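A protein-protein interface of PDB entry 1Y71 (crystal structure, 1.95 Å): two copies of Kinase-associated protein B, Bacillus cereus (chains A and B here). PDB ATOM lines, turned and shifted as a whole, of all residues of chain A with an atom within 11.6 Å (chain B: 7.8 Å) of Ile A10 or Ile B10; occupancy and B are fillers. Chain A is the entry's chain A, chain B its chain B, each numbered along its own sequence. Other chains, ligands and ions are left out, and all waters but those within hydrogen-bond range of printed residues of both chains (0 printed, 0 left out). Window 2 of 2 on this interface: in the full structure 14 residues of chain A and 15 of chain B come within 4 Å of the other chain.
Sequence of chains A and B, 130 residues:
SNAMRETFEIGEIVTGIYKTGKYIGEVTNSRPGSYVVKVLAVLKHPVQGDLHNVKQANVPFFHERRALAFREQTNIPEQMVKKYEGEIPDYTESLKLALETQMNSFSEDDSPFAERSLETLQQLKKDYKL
OE2 of Glu B26 sits close to OE2 of Glu A26, at 3.1 Å. The side-chain carboxylate (OE2) of Glu B26 sits close to the backbone carbonyl oxygen (O) of Gly A11 (2.4 Å). The side-chain carboxylate (OE2) of Glu A26 sits close to the backbone carbonyl oxygen (O) of Gly B11, 2.4 Å away.
N of Gly A11 lies within hydrogen-bond range of O of Val A27, 2.7 Å away. The backbone NH (N) of Lys A38 is in hydrogen-bond range of the backbone carbonyl oxygen (O) of Glu A26, 2.8 Å away. N of Gly B11 sits at hydrogen-bond distance from O of Val B27, 2.8 Å away.
Among the printed residues, pairs that only touch across the chains: Ile A10 with Ile B10, Gly A11 with Gly B11, Ile A13 with Glu B26 and Glu A26 with Ile B13.
Ile A10 touches just one residue of chain B: Ile B10. Printed residues of chain B within 4 Å of Gly A11: Gly B11 and Glu B26. Of the printed residues of chain B, Ile A13 touches Glu B26. Of the printed residues of chain B, Glu A26 touches Gly B11 (2.4 Å), Ile B13 (3.7 Å) and Glu B26 (3.1 Å). No residue of chain A comes within 4 Å of Glu B9. Ile B10 touches just one residue of chain A: Ile A10 (3.7 Å). Gly B11 touches just these residues of chain A: Gly A11 (3.9 Å) and Glu A26 (2.4 Å). Printed residues of chain A within 4 Å of Ile B13: Glu A26. Printed residues of chain A within 4 Å of Glu B26: Gly A11, Ile A13 and Glu A26. No residue of chain A comes within 4 Å of Val B27. Thr B28 touches none of the printed residues of chain A. No residue of chain A comes within 4 Å of Asn B29. The nearest residue of chain B that does not touch Ile A10 is Gly B11 (5.2 Å). The nearest residue of chain A that does not touch Ile B10 is Gly A11 (4.9 Å).
Printed residues of chain A that touch a printed residue of chain B: Ile A10, Gly A11, Ile A13 and Glu A26. Along chain A the printed residues that touch a printed residue of chain B span positions 10 to 26. Among the printed residues, 7 pairs touch across the chains. Among the printed residues, no Asp or Glu carboxylate lies within 4 Å of a Lys or Arg side-chain nitrogen of the other chain.
Gly A11 touches its own counterpart, Gly B11. Gly A11 touches Glu B26, and with the chains exchanged Glu A26 touches Gly B11. Ile A13 touches Glu B26, and with the chains exchanged Glu A26 touches Ile B13. Glu B26 touches its own counterpart, Glu A26. Of the 7 pairs that touch across the chains among the printed residues, 7 have their exchanged pair printed and touching as well.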
ATOM      1  N   THR A   7      21.334  26.258  11.914  1.00  0.00           N
ATOM      2  CA  THR A   7      22.292  25.532  11.020  1.00  0.00           C
ATOM      3  C   THR A   7      22.624  26.339   9.759  1.00  0.00           C
ATOM      4  O   THR A   7      21.917  26.265   8.747  1.00  0.00           O
ATOM      5  CB  THR A   7      21.769  24.130  10.637  1.00  0.00           C
ATOM      6  OG1 THR A   7      21.664  23.331  11.816  1.00  0.00           O
ATOM      7  CG2 THR A   7      22.712  23.415   9.640  1.00  0.00           C
ATOM      8  N   PHE A   8      23.713  27.094   9.824  1.00  0.00           N
ATOM      9  CA  PHE A   8      24.192  27.851   8.672  1.00  0.00           C
ATOM     10  C   PHE A   8      24.464  26.958   7.474  1.00  0.00           C
ATOM     11  O   PHE A   8      24.984  25.845   7.610  1.00  0.00           O
ATOM     12  CB  PHE A   8      25.429  28.676   9.033  1.00  0.00           C
ATOM     13  CG  PHE A   8      25.261  29.491  10.285  1.00  0.00           C
ATOM     14  CD1 PHE A   8      26.092  29.292  11.362  1.00  0.00           C
ATOM     15  CD2 PHE A   8      24.234  30.435  10.392  1.00  0.00           C
ATOM     16  CE1 PHE A   8      25.927  30.018  12.548  1.00  0.00           C
ATOM     17  CE2 PHE A   8      24.067  31.175  11.556  1.00  0.00           C
ATOM     18  CZ  PHE A   8      24.918  30.956  12.652  1.00  0.00           C
ATOM     19  N   GLU A   9      24.063  27.468   6.311  1.00  0.00           N
ATOM     20  CA  GLU A   9      24.216  26.794   5.047  1.00  0.00           C
ATOM     21  C   GLU A   9      25.597  27.139   4.511  1.00  0.00           C
ATOM     22  O   GLU A   9      26.170  28.195   4.856  1.00  0.00           O
ATOM     23  CB  GLU A   9      23.116  27.233   4.061  1.00  0.00           C
ATOM     24  CG  GLU A   9      21.648  27.048   4.593  1.00  0.00           C
ATOM     25  CD  GLU A   9      20.578  26.800   3.499  1.00  0.00           C
ATOM     26  OE1 GLU A   9      19.358  26.723   3.851  1.00  0.00           O
ATOM     27  OE2 GLU A   9      20.934  26.667   2.297  1.00  0.00           O
ATOM     28  N   ILE A  10      26.114  26.248   3.660  1.00  0.00           N
ATOM     29  CA  ILE A  10      27.381  26.447   2.984  1.00  0.00           C
ATOM     30  C   ILE A  10      27.252  27.736   2.184  1.00  0.00           C
ATOM     31  O   ILE A  10      26.256  27.957   1.492  1.00  0.00           O
ATOM     32  CB  ILE A  10      27.759  25.232   2.077  1.00  0.00           C
ATOM     33  CG1 ILE A  10      28.241  24.058   2.937  1.00  0.00           C
ATOM     34  CG2 ILE A  10      28.824  25.611   1.040  1.00  0.00           C
ATOM     35  CD1 ILE A  10      28.505  22.772   2.127  1.00  0.00           C
ATOM     36  N   GLY A  11      28.240  28.605   2.325  1.00  0.00           N
ATOM     37  CA  GLY A  11      28.193  29.898   1.672  1.00  0.00           C
ATOM     38  C   GLY A  11      27.826  31.016   2.628  1.00  0.00           C
ATOM     39  O   GLY A  11      28.053  32.172   2.332  1.00  0.00           O
ATOM     40  N   GLU A  12      27.267  30.690   3.794  1.00  0.00           N
ATOM     41  CA  GLU A  12      26.879  31.736   4.731  1.00  0.00           C
ATOM     42  C   GLU A  12      28.051  32.636   5.229  1.00  0.00           C
ATOM     43  O   GLU A  12      29.123  32.155   5.587  1.00  0.00           O
ATOM     44  CB  GLU A  12      26.115  31.142   5.916  1.00  0.00           C
ATOM     45  CG  GLU A  12      25.487  32.193   6.791  1.00  0.00           C
ATOM     46  CD  GLU A  12      24.371  32.924   6.079  1.00  0.00           C
ATOM     47  OE1 GLU A  12      23.332  32.283   5.790  1.00  0.00           O
ATOM     48  OE2 GLU A  12      24.539  34.129   5.797  1.00  0.00           O
ATOM     49  N   ILE A  13      27.827  33.937   5.242  1.00  0.00           N
ATOM     50  CA  ILE A  13      28.833  34.881   5.744  1.00  0.00           C
ATOM     51  C   ILE A  13      28.616  35.006   7.248  1.00  0.00           C
ATOM     52  O   ILE A  13      27.497  35.288   7.692  1.00  0.00           O
ATOM     53  CB  ILE A  13      28.763  36.257   5.039  1.00  0.00           C
ATOM     54  CG1 ILE A  13      28.879  36.119   3.483  1.00  0.00           C
ATOM     55  CG2 ILE A  13      29.783  37.247   5.667  1.00  0.00           C
ATOM     56  CD1 ILE A  13      30.195  35.551   3.005  1.00  0.00           C
ATOM     57  N   VAL A  14      29.672  34.767   8.019  1.00  0.00           N
ATOM     58  CA  VAL A  14      29.561  34.643   9.473  1.00  0.00           C
ATOM     59  C   VAL A  14      30.731  35.335  10.162  1.00  0.00           C
ATOM     60  O   VAL A  14      31.722  35.700   9.521  1.00  0.00           O
ATOM     61  CB  VAL A  14      29.551  33.139   9.949  1.00  0.00           C
ATOM     62  CG1 VAL A  14      28.333  32.396   9.392  1.00  0.00           C
ATOM     63  CG2 VAL A  14      30.867  32.425   9.579  1.00  0.00           C
ATOM     64  N   GLY A  25      34.149  35.443   8.014  1.00  0.00           N
ATOM     65  CA  GLY A  25      34.396  34.381   7.041  1.00  0.00           C
ATOM     66  C   GLY A  25      33.136  33.821   6.425  1.00  0.00           C
ATOM     67  O   GLY A  25      32.046  34.453   6.499  1.00  0.00           O
ATOM     68  N   GLU A  26      33.312  32.656   5.784  1.00  0.00           N
ATOM     69  CA  GLU A  26      32.288  32.002   5.013  1.00  0.00           C
ATOM     70  C   GLU A  26      32.280  30.517   5.374  1.00  0.00           C
ATOM     71  O   GLU A  26      33.333  29.871   5.367  1.00  0.00           O
ATOM     72  CB  GLU A  26      32.624  32.193   3.515  1.00  0.00           C
ATOM     73  CG  GLU A  26      31.605  31.734   2.588  1.00  0.00           C
ATOM     74  CD  GLU A  26      32.163  31.456   1.194  1.00  0.00           C
ATOM     75  OE1 GLU A  26      33.284  31.905   0.840  1.00  0.00           O
ATOM     76  OE2 GLU A  26      31.466  30.739   0.463  1.00  0.00           O
ATOM     77  N   VAL A  27      31.099  29.998   5.720  1.00  0.00           N
ATOM     78  CA  VAL A  27      30.908  28.572   6.012  1.00  0.00           C
ATOM     79  C   VAL A  27      31.159  27.778   4.721  1.00  0.00           C
ATOM     80  O   VAL A  27      30.551  28.043   3.672  1.00  0.00           O
ATOM     81  CB  VAL A  27      29.471  28.283   6.513  1.00  0.00           C
ATOM     82  CG1 VAL A  27      29.263  26.746   6.725  1.00  0.00           C
ATOM     83  CG2 VAL A  27      29.180  29.047   7.798  1.00  0.00           C
ATOM     84  N   THR A  28      32.074  26.822   4.794  1.00  0.00           N
ATOM     85  CA  THR A  28      32.378  25.972   3.628  1.00  0.00           C
ATOM     86  C   THR A  28      32.020  24.521   3.865  1.00  0.00           C
ATOM     87  O   THR A  28      31.903  23.751   2.908  1.00  0.00           O
ATOM     88  CB  THR A  28      33.853  26.049   3.225  1.00  0.00           C
ATOM     89  OG1 THR A  28      34.641  25.707   4.363  1.00  0.00           O
ATOM     90  CG2 THR A  28      34.212  27.493   2.725  1.00  0.00           C
ATOM     91  N   ASN A  29      31.868  24.171   5.143  1.00  0.00           N
ATOM     92  CA  ASN A  29      31.422  22.854   5.561  1.00  0.00           C
ATOM     93  C   ASN A  29      30.754  22.870   6.944  1.00  0.00           C
ATOM     94  O   ASN A  29      30.917  23.803   7.741  1.00  0.00           O
ATOM     95  CB  ASN A  29      32.583  21.845   5.529  1.00  0.00           C
ATOM     96  CG  ASN A  29      32.109  20.420   5.278  1.00  0.00           C
ATOM     97  OD1 ASN A  29      30.930  20.171   4.951  1.00  0.00           O
ATOM     98  ND2 ASN A  29      33.026  19.471   5.424  1.00  0.00           N
ATOM     99  N   SER A  30      29.998  21.818   7.222  1.00  0.00           N
ATOM    100  CA  SER A  30      29.188  21.743   8.420  1.00  0.00           C
ATOM    101  C   SER A  30      29.181  20.307   8.927  1.00  0.00           C
ATOM    102  O   SER A  30      29.083  19.362   8.132  1.00  0.00           O
ATOM    103  CB  SER A  30      27.764  22.200   8.097  1.00  0.00           C
ATOM    104  OG  SER A  30      26.895  22.022   9.195  1.00  0.00           O
ATOM    105  N   ARG A  31      29.315  20.157  10.243  1.00  0.00           N
ATOM    106  CA  ARG A  31      29.170  18.857  10.921  1.00  0.00           C
ATOM    107  C   ARG A  31      28.596  19.112  12.318  1.00  0.00           C
ATOM    108  O   ARG A  31      28.686  20.243  12.809  1.00  0.00           O
ATOM    109  CB  ARG A  31      30.518  18.118  11.004  1.00  0.00           C
ATOM    110  CG  ARG A  31      31.664  18.916  11.640  1.00  0.00           C
ATOM    111  CD  ARG A  31      32.840  18.009  11.989  1.00  0.00           C
ATOM    112  NE  ARG A  31      33.626  18.538  13.107  1.00  0.00           N
ATOM    113  CZ  ARG A  31      34.639  17.906  13.701  1.00  0.00           C
ATOM    114  NH1 ARG A  31      35.017  16.689  13.300  1.00  0.00           N
ATOM    115  NH2 ARG A  31      35.277  18.493  14.708  1.00  0.00           N
ATOM    116  N   SER A  34      29.878  21.987  14.904  1.00  0.00           N
ATOM    117  CA  SER A  34      31.031  22.688  14.327  1.00  0.00           C
ATOM    118  C   SER A  34      30.797  23.197  12.904  1.00  0.00           C
ATOM    119  O   SER A  34      29.970  22.660  12.173  1.00  0.00           O
ATOM    120  CB  SER A  34      32.240  21.757  14.322  1.00  0.00           C
ATOM    121  OG  SER A  34      33.431  22.491  14.448  1.00  0.00           O
ATOM    122  N   TYR A  35      31.540  24.237  12.525  1.00  0.00           N
ATOM    123  CA  TYR A  35      31.594  24.695  11.127  1.00  0.00           C
ATOM    124  C   TYR A  35      33.039  24.875  10.673  1.00  0.00           C
ATOM    125  O   TYR A  35      33.877  25.367  11.438  1.00  0.00           O
ATOM    126  CB  TYR A  35      30.872  26.038  10.942  1.00  0.00           C
ATOM    127  CG  TYR A  35      29.381  26.013  11.224  1.00  0.00           C
ATOM    128  CD1 TYR A  35      28.473  25.674  10.227  1.00  0.00           C
ATOM    129  CD2 TYR A  35      28.885  26.340  12.494  1.00  0.00           C
ATOM    130  CE1 TYR A  35      27.103  25.648  10.483  1.00  0.00           C
ATOM    131  CE2 TYR A  35      27.517  26.334  12.759  1.00  0.00           C
ATOM    132  CZ  TYR A  35      26.639  25.979  11.761  1.00  0.00           C
ATOM    133  OH  TYR A  35      25.291  25.970  12.022  1.00  0.00           O
ATOM    134  N   VAL A  36      33.308  24.496   9.429  1.00  0.00           N
ATOM    135  CA  VAL A  36      34.535  24.917   8.751  1.00  0.00           C
ATOM    136  C   VAL A  36      34.300  26.298   8.183  1.00  0.00           C
ATOM    137  O   VAL A  36      33.374  26.511   7.404  1.00  0.00           O
ATOM    138  CB  VAL A  36      34.943  23.922   7.649  1.00  0.00           C
ATOM    139  CG1 VAL A  36      36.173  24.422   6.874  1.00  0.00           C
ATOM    140  CG2 VAL A  36      35.181  22.530   8.275  1.00  0.00           C
ATOM    141  N   VAL A  37      35.146  27.238   8.590  1.00  0.00           N
ATOM    142  CA  VAL A  37      35.022  28.613   8.170  1.00  0.00           C
ATOM    143  C   VAL A  37      36.257  29.020   7.436  1.00  0.00           C
ATOM    144  O   VAL A  37      37.406  28.827   7.919  1.00  0.00           O
ATOM    145  CB  VAL A  37      34.736  29.600   9.368  1.00  0.00           C
ATOM    146  CG1 VAL A  37      34.608  31.102   8.864  1.00  0.00           C
ATOM    147  CG2 VAL A  37      33.459  29.199  10.105  1.00  0.00           C
ATOM    148  N   LYS A  38      36.007  29.591   6.263  1.00  0.00           N
ATOM    149  CA  LYS A  38      37.063  30.198   5.451  1.00  0.00           C
ATOM    150  C   LYS A  38      37.187  31.676   5.794  1.00  0.00           C
ATOM    151  O   LYS A  38      36.240  32.446   5.630  1.00  0.00           O
ATOM    152  CB  LYS A  38      36.751  29.989   3.955  1.00  0.00           C
ATOM    153  CG  LYS A  38      37.764  30.629   2.984  1.00  0.00           C
ATOM    154  CD  LYS A  38      37.265  30.592   1.535  1.00  0.00           C
ATOM    155  CE  LYS A  38      37.011  29.172   1.050  1.00  0.00           C
ATOM    156  NZ  LYS A  38      36.569  29.044  -0.409  1.00  0.00           N
ATOM    157  N   LEU A  40      37.957  35.525   5.782  1.00  0.00           N
ATOM    158  CA  LEU A  40      37.965  36.635   4.825  1.00  0.00           C
ATOM    159  C   LEU A  40      38.498  37.981   5.417  1.00  0.00           C
ATOM    160  O   LEU A  40      38.981  38.838   4.676  1.00  0.00           O
ATOM    161  CB  LEU A  40      36.540  36.853   4.284  1.00  0.00           C
ATOM    162  CG  LEU A  40      36.000  35.615   3.555  1.00  0.00           C
ATOM    163  CD1 LEU A  40      34.555  35.881   3.123  1.00  0.00           C
ATOM    164  CD2 LEU A  40      36.951  35.169   2.348  1.00  0.00           C
ATOM    165  N   GLN A  73      41.151  27.952   6.214  1.00  0.00           N
ATOM    166  CA  GLN A  73      39.922  27.283   6.592  1.00  0.00           C
ATOM    167  C   GLN A  73      40.081  26.627   7.964  1.00  0.00           C
ATOM    168  O   GLN A  73      41.017  25.824   8.195  1.00  0.00           O
ATOM    169  CB  GLN A  73      39.501  26.278   5.533  1.00  0.00           C
ATOM    170  CG  GLN A  73      39.292  26.963   4.174  1.00  0.00           C
ATOM    171  CD  GLN A  73      38.257  26.302   3.318  1.00  0.00           C
ATOM    172  OE1 GLN A  73      37.272  25.755   3.810  1.00  0.00           O
ATOM    173  NE2 GLN A  73      38.447  26.389   2.008  1.00  0.00           N
ATOM    174  N   VAL A  81      30.109  30.622  16.325  1.00  0.00           N
ATOM    175  CA  VAL A  81      29.822  31.083  14.958  1.00  0.00           C
ATOM    176  C   VAL A  81      28.482  31.841  14.892  1.00  0.00           C
ATOM    177  O   VAL A  81      27.466  31.344  15.357  1.00  0.00           O
ATOM    178  CB  VAL A  81      29.836  29.878  13.943  1.00  0.00           C
ATOM    179  CG1 VAL A  81      29.512  30.350  12.517  1.00  0.00           C
ATOM    180  CG2 VAL A  81      31.170  29.184  13.975  1.00  0.00           C
ATOM    181  N   LYS A  83      25.832  34.435  12.288  1.00  0.00           N
ATOM    182  CA  LYS A  83      25.553  35.109  11.036  1.00  0.00           C
ATOM    183  C   LYS A  83      26.129  36.524  11.072  1.00  0.00           C
ATOM    184  O   LYS A  83      26.069  37.198  12.101  1.00  0.00           O
ATOM    185  CB  LYS A  83      24.046  35.118  10.755  1.00  0.00           C
ATOM    186  CG  LYS A  83      23.704  35.390   9.318  1.00  0.00           C
ATOM    187  CD  LYS A  83      22.191  35.334   9.105  1.00  0.00           C
ATOM    188  CE  LYS A  83      21.827  36.118   7.851  1.00  0.00           C
ATOM    189  NZ  LYS A  83      22.156  35.405   6.596  1.00  0.00           N
ATOM    190  N   PHE B   8      31.185  26.742 -11.291  1.00  0.00           N
ATOM    191  CA  PHE B   8      31.403  27.416 -10.009  1.00  0.00           C
ATOM    192  C   PHE B   8      30.462  26.854  -8.957  1.00  0.00           C
ATOM    193  O   PHE B   8      29.279  26.677  -9.230  1.00  0.00           O
ATOM    194  CB  PHE B   8      31.183  28.924 -10.167  1.00  0.00           C
ATOM    195  CG  PHE B   8      32.056  29.564 -11.213  1.00  0.00           C
ATOM    196  CD1 PHE B   8      31.502  30.071 -12.378  1.00  0.00           C
ATOM    197  CD2 PHE B   8      33.430  29.662 -11.035  1.00  0.00           C
ATOM    198  CE1 PHE B   8      32.314  30.667 -13.354  1.00  0.00           C
ATOM    199  CE2 PHE B   8      34.241  30.250 -11.998  1.00  0.00           C
ATOM    200  CZ  PHE B   8      33.688  30.755 -13.148  1.00  0.00           C
ATOM    201  N   GLU B   9      30.982  26.556  -7.767  1.00  0.00           N
ATOM    202  CA  GLU B   9      30.123  26.049  -6.690  1.00  0.00           C
ATOM    203  C   GLU B   9      29.569  27.150  -5.785  1.00  0.00           C
ATOM    204  O   GLU B   9      30.095  28.267  -5.736  1.00  0.00           O
ATOM    205  CB  GLU B   9      30.793  24.915  -5.897  1.00  0.00           C
ATOM    206  CG  GLU B   9      32.054  25.305  -5.112  1.00  0.00           C
ATOM    207  CD  GLU B   9      32.897  24.091  -4.686  1.00  0.00           C
ATOM    208  OE1 GLU B   9      32.535  23.387  -3.706  1.00  0.00           O
ATOM    209  OE2 GLU B   9      33.941  23.852  -5.347  1.00  0.00           O
ATOM    210  N   ILE B  10      28.455  26.835  -5.129  1.00  0.00           N
ATOM    211  CA  ILE B  10      27.847  27.712  -4.137  1.00  0.00           C
ATOM    212  C   ILE B  10      28.858  28.041  -3.053  1.00  0.00           C
ATOM    213  O   ILE B  10      29.503  27.138  -2.488  1.00  0.00           O
ATOM    214  CB  ILE B  10      26.574  27.083  -3.531  1.00  0.00           C
ATOM    215  CG1 ILE B  10      25.413  27.237  -4.508  1.00  0.00           C
ATOM    216  CG2 ILE B  10      26.214  27.731  -2.200  1.00  0.00           C
ATOM    217  CD1 ILE B  10      24.076  26.675  -3.984  1.00  0.00           C
ATOM    218  N   GLY B  11      28.983  29.333  -2.767  1.00  0.00           N
ATOM    219  CA  GLY B  11      29.948  29.799  -1.795  1.00  0.00           C
ATOM    220  C   GLY B  11      31.203  30.302  -2.485  1.00  0.00           C
ATOM    221  O   GLY B  11      32.017  30.989  -1.883  1.00  0.00           O
ATOM    222  N   GLU B  12      31.370  29.963  -3.755  1.00  0.00           N
ATOM    223  CA  GLU B  12      32.594  30.361  -4.455  1.00  0.00           C
ATOM    224  C   GLU B  12      32.686  31.877  -4.608  1.00  0.00           C
ATOM    225  O   GLU B  12      31.719  32.520  -5.027  1.00  0.00           O
ATOM    226  CB  GLU B  12      32.682  29.646  -5.795  1.00  0.00           C
ATOM    227  CG  GLU B  12      33.849  30.083  -6.668  1.00  0.00           C
ATOM    228  CD  GLU B  12      34.263  29.004  -7.655  1.00  0.00           C
ATOM    229  OE1 GLU B  12      35.247  29.242  -8.373  1.00  0.00           O
ATOM    230  OE2 GLU B  12      33.618  27.929  -7.709  1.00  0.00           O
ATOM    231  N   ILE B  13      33.850  32.437  -4.275  1.00  0.00           N
ATOM    232  CA  ILE B  13      34.148  33.859  -4.509  1.00  0.00           C
ATOM    233  C   ILE B  13      34.564  34.077  -5.959  1.00  0.00           C
ATOM    234  O   ILE B  13      35.456  33.381  -6.473  1.00  0.00           O
ATOM    235  CB  ILE B  13      35.230  34.411  -3.545  1.00  0.00           C
ATOM    236  CG1 ILE B  13      34.841  34.109  -2.095  1.00  0.00           C
ATOM    237  CG2 ILE B  13      35.409  35.918  -3.749  1.00  0.00           C
ATOM    238  CD1 ILE B  13      33.418  34.625  -1.718  1.00  0.00           C
ATOM    239  N   GLU B  26      29.752  36.512  -4.360  1.00  0.00           N
ATOM    240  CA  GLU B  26      29.713  35.120  -3.958  1.00  0.00           C
ATOM    241  C   GLU B  26      28.621  34.380  -4.740  1.00  0.00           C
ATOM    242  O   GLU B  26      27.506  34.879  -4.863  1.00  0.00           O
ATOM    243  CB  GLU B  26      29.483  35.050  -2.435  1.00  0.00           C
ATOM    244  CG  GLU B  26      29.418  33.647  -1.890  1.00  0.00           C
ATOM    245  CD  GLU B  26      28.860  33.592  -0.493  1.00  0.00           C
ATOM    246  OE1 GLU B  26      28.360  34.621   0.024  1.00  0.00           O
ATOM    247  OE2 GLU B  26      28.909  32.487   0.078  1.00  0.00           O
ATOM    248  N   VAL B  27      28.953  33.237  -5.321  1.00  0.00           N
ATOM    249  CA  VAL B  27      27.941  32.433  -6.009  1.00  0.00           C
ATOM    250  C   VAL B  27      26.951  31.909  -4.963  1.00  0.00           C
ATOM    251  O   VAL B  27      27.358  31.275  -3.991  1.00  0.00           O
ATOM    252  CB  VAL B  27      28.582  31.283  -6.824  1.00  0.00           C
ATOM    253  CG1 VAL B  27      27.509  30.313  -7.382  1.00  0.00           C
ATOM    254  CG2 VAL B  27      29.460  31.861  -7.958  1.00  0.00           C
ATOM    255  N   THR B  28      25.671  32.225  -5.133  1.00  0.00           N
ATOM    256  CA  THR B  28      24.643  31.738  -4.206  1.00  0.00           C
ATOM    257  C   THR B  28      23.638  30.757  -4.849  1.00  0.00           C
ATOM    258  O   THR B  28      22.870  30.102  -4.146  1.00  0.00           O
ATOM    259  CB  THR B  28      23.882  32.884  -3.497  1.00  0.00           C
ATOM    260  OG1 THR B  28      23.112  33.605  -4.449  1.00  0.00           O
ATOM    261  CG2 THR B  28      24.850  33.863  -2.789  1.00  0.00           C
ATOM    262  N   ASN B  29      23.645  30.658  -6.170  1.00  0.00           N
ATOM    263  CA  ASN B  29      22.802  29.679  -6.872  1.00  0.00           C
ATOM    264  C   ASN B  29      23.289  29.552  -8.315  1.00  0.00           C
ATOM    265  O   ASN B  29      23.835  30.505  -8.884  1.00  0.00           O
ATOM    266  CB  ASN B  29      21.311  30.093  -6.822  1.00  0.00           C
ATOM    267  CG  ASN B  29      20.325  28.921  -7.054  1.00  0.00           C
ATOM    268  OD1 ASN B  29      20.609  27.748  -6.755  1.00  0.00           O
ATOM    269  ND2 ASN B  29      19.140  29.255  -7.571  1.00  0.00           N
ATOM    270  N   SER B  30      23.093  28.360  -8.877  1.00  0.00           N
ATOM    271  CA  SER B  30      23.361  28.075 -10.277  1.00  0.00           C
ATOM    272  C   SER B  30      22.041  27.812 -10.991  1.00  0.00           C
ATOM    273  O   SER B  30      21.000  27.552 -10.365  1.00  0.00           O
ATOM    274  CB  SER B  30      24.238  26.825 -10.434  1.00  0.00           C
ATOM    275  OG  SER B  30      25.451  26.901  -9.702  1.00  0.00           O
ATOM    276  N   TYR B  35      24.713  32.342 -13.141  1.00  0.00           N
ATOM    277  CA  TYR B  35      24.881  32.236 -11.707  1.00  0.00           C
ATOM    278  C   TYR B  35      24.215  33.412 -11.051  1.00  0.00           C
ATOM    279  O   TYR B  35      24.276  34.521 -11.568  1.00  0.00           O
ATOM    280  CB  TYR B  35      26.369  32.234 -11.351  1.00  0.00           C
ATOM    281  CG  TYR B  35      27.060  31.008 -11.877  1.00  0.00           C
ATOM    282  CD1 TYR B  35      27.027  29.817 -11.152  1.00  0.00           C
ATOM    283  CD2 TYR B  35      27.725  31.027 -13.123  1.00  0.00           C
ATOM    284  CE1 TYR B  35      27.620  28.677 -11.624  1.00  0.00           C
ATOM    285  CE2 TYR B  35      28.331  29.874 -13.612  1.00  0.00           C
ATOM    286  CZ  TYR B  35      28.275  28.699 -12.845  1.00  0.00           C
ATOM    287  OH  TYR B  35      28.869  27.536 -13.290  1.00  0.00           O
ATOM    288  N   VAL B  36      23.602  33.162  -9.893  1.00  0.00           N
ATOM    289  CA  VAL B  36      23.159  34.230  -9.034  1.00  0.00           C
ATOM    290  C   VAL B  36      24.399  34.586  -8.208  1.00  0.00           C
ATOM    291  O   VAL B  36      25.024  33.700  -7.596  1.00  0.00           O
ATOM    292  CB  VAL B  36      21.951  33.830  -8.124  1.00  0.00           C
ATOM    293  CG1 VAL B  36      21.518  35.009  -7.317  1.00  0.00           C
ATOM    294  CG2 VAL B  36      20.758  33.331  -8.995  1.00  0.00           C
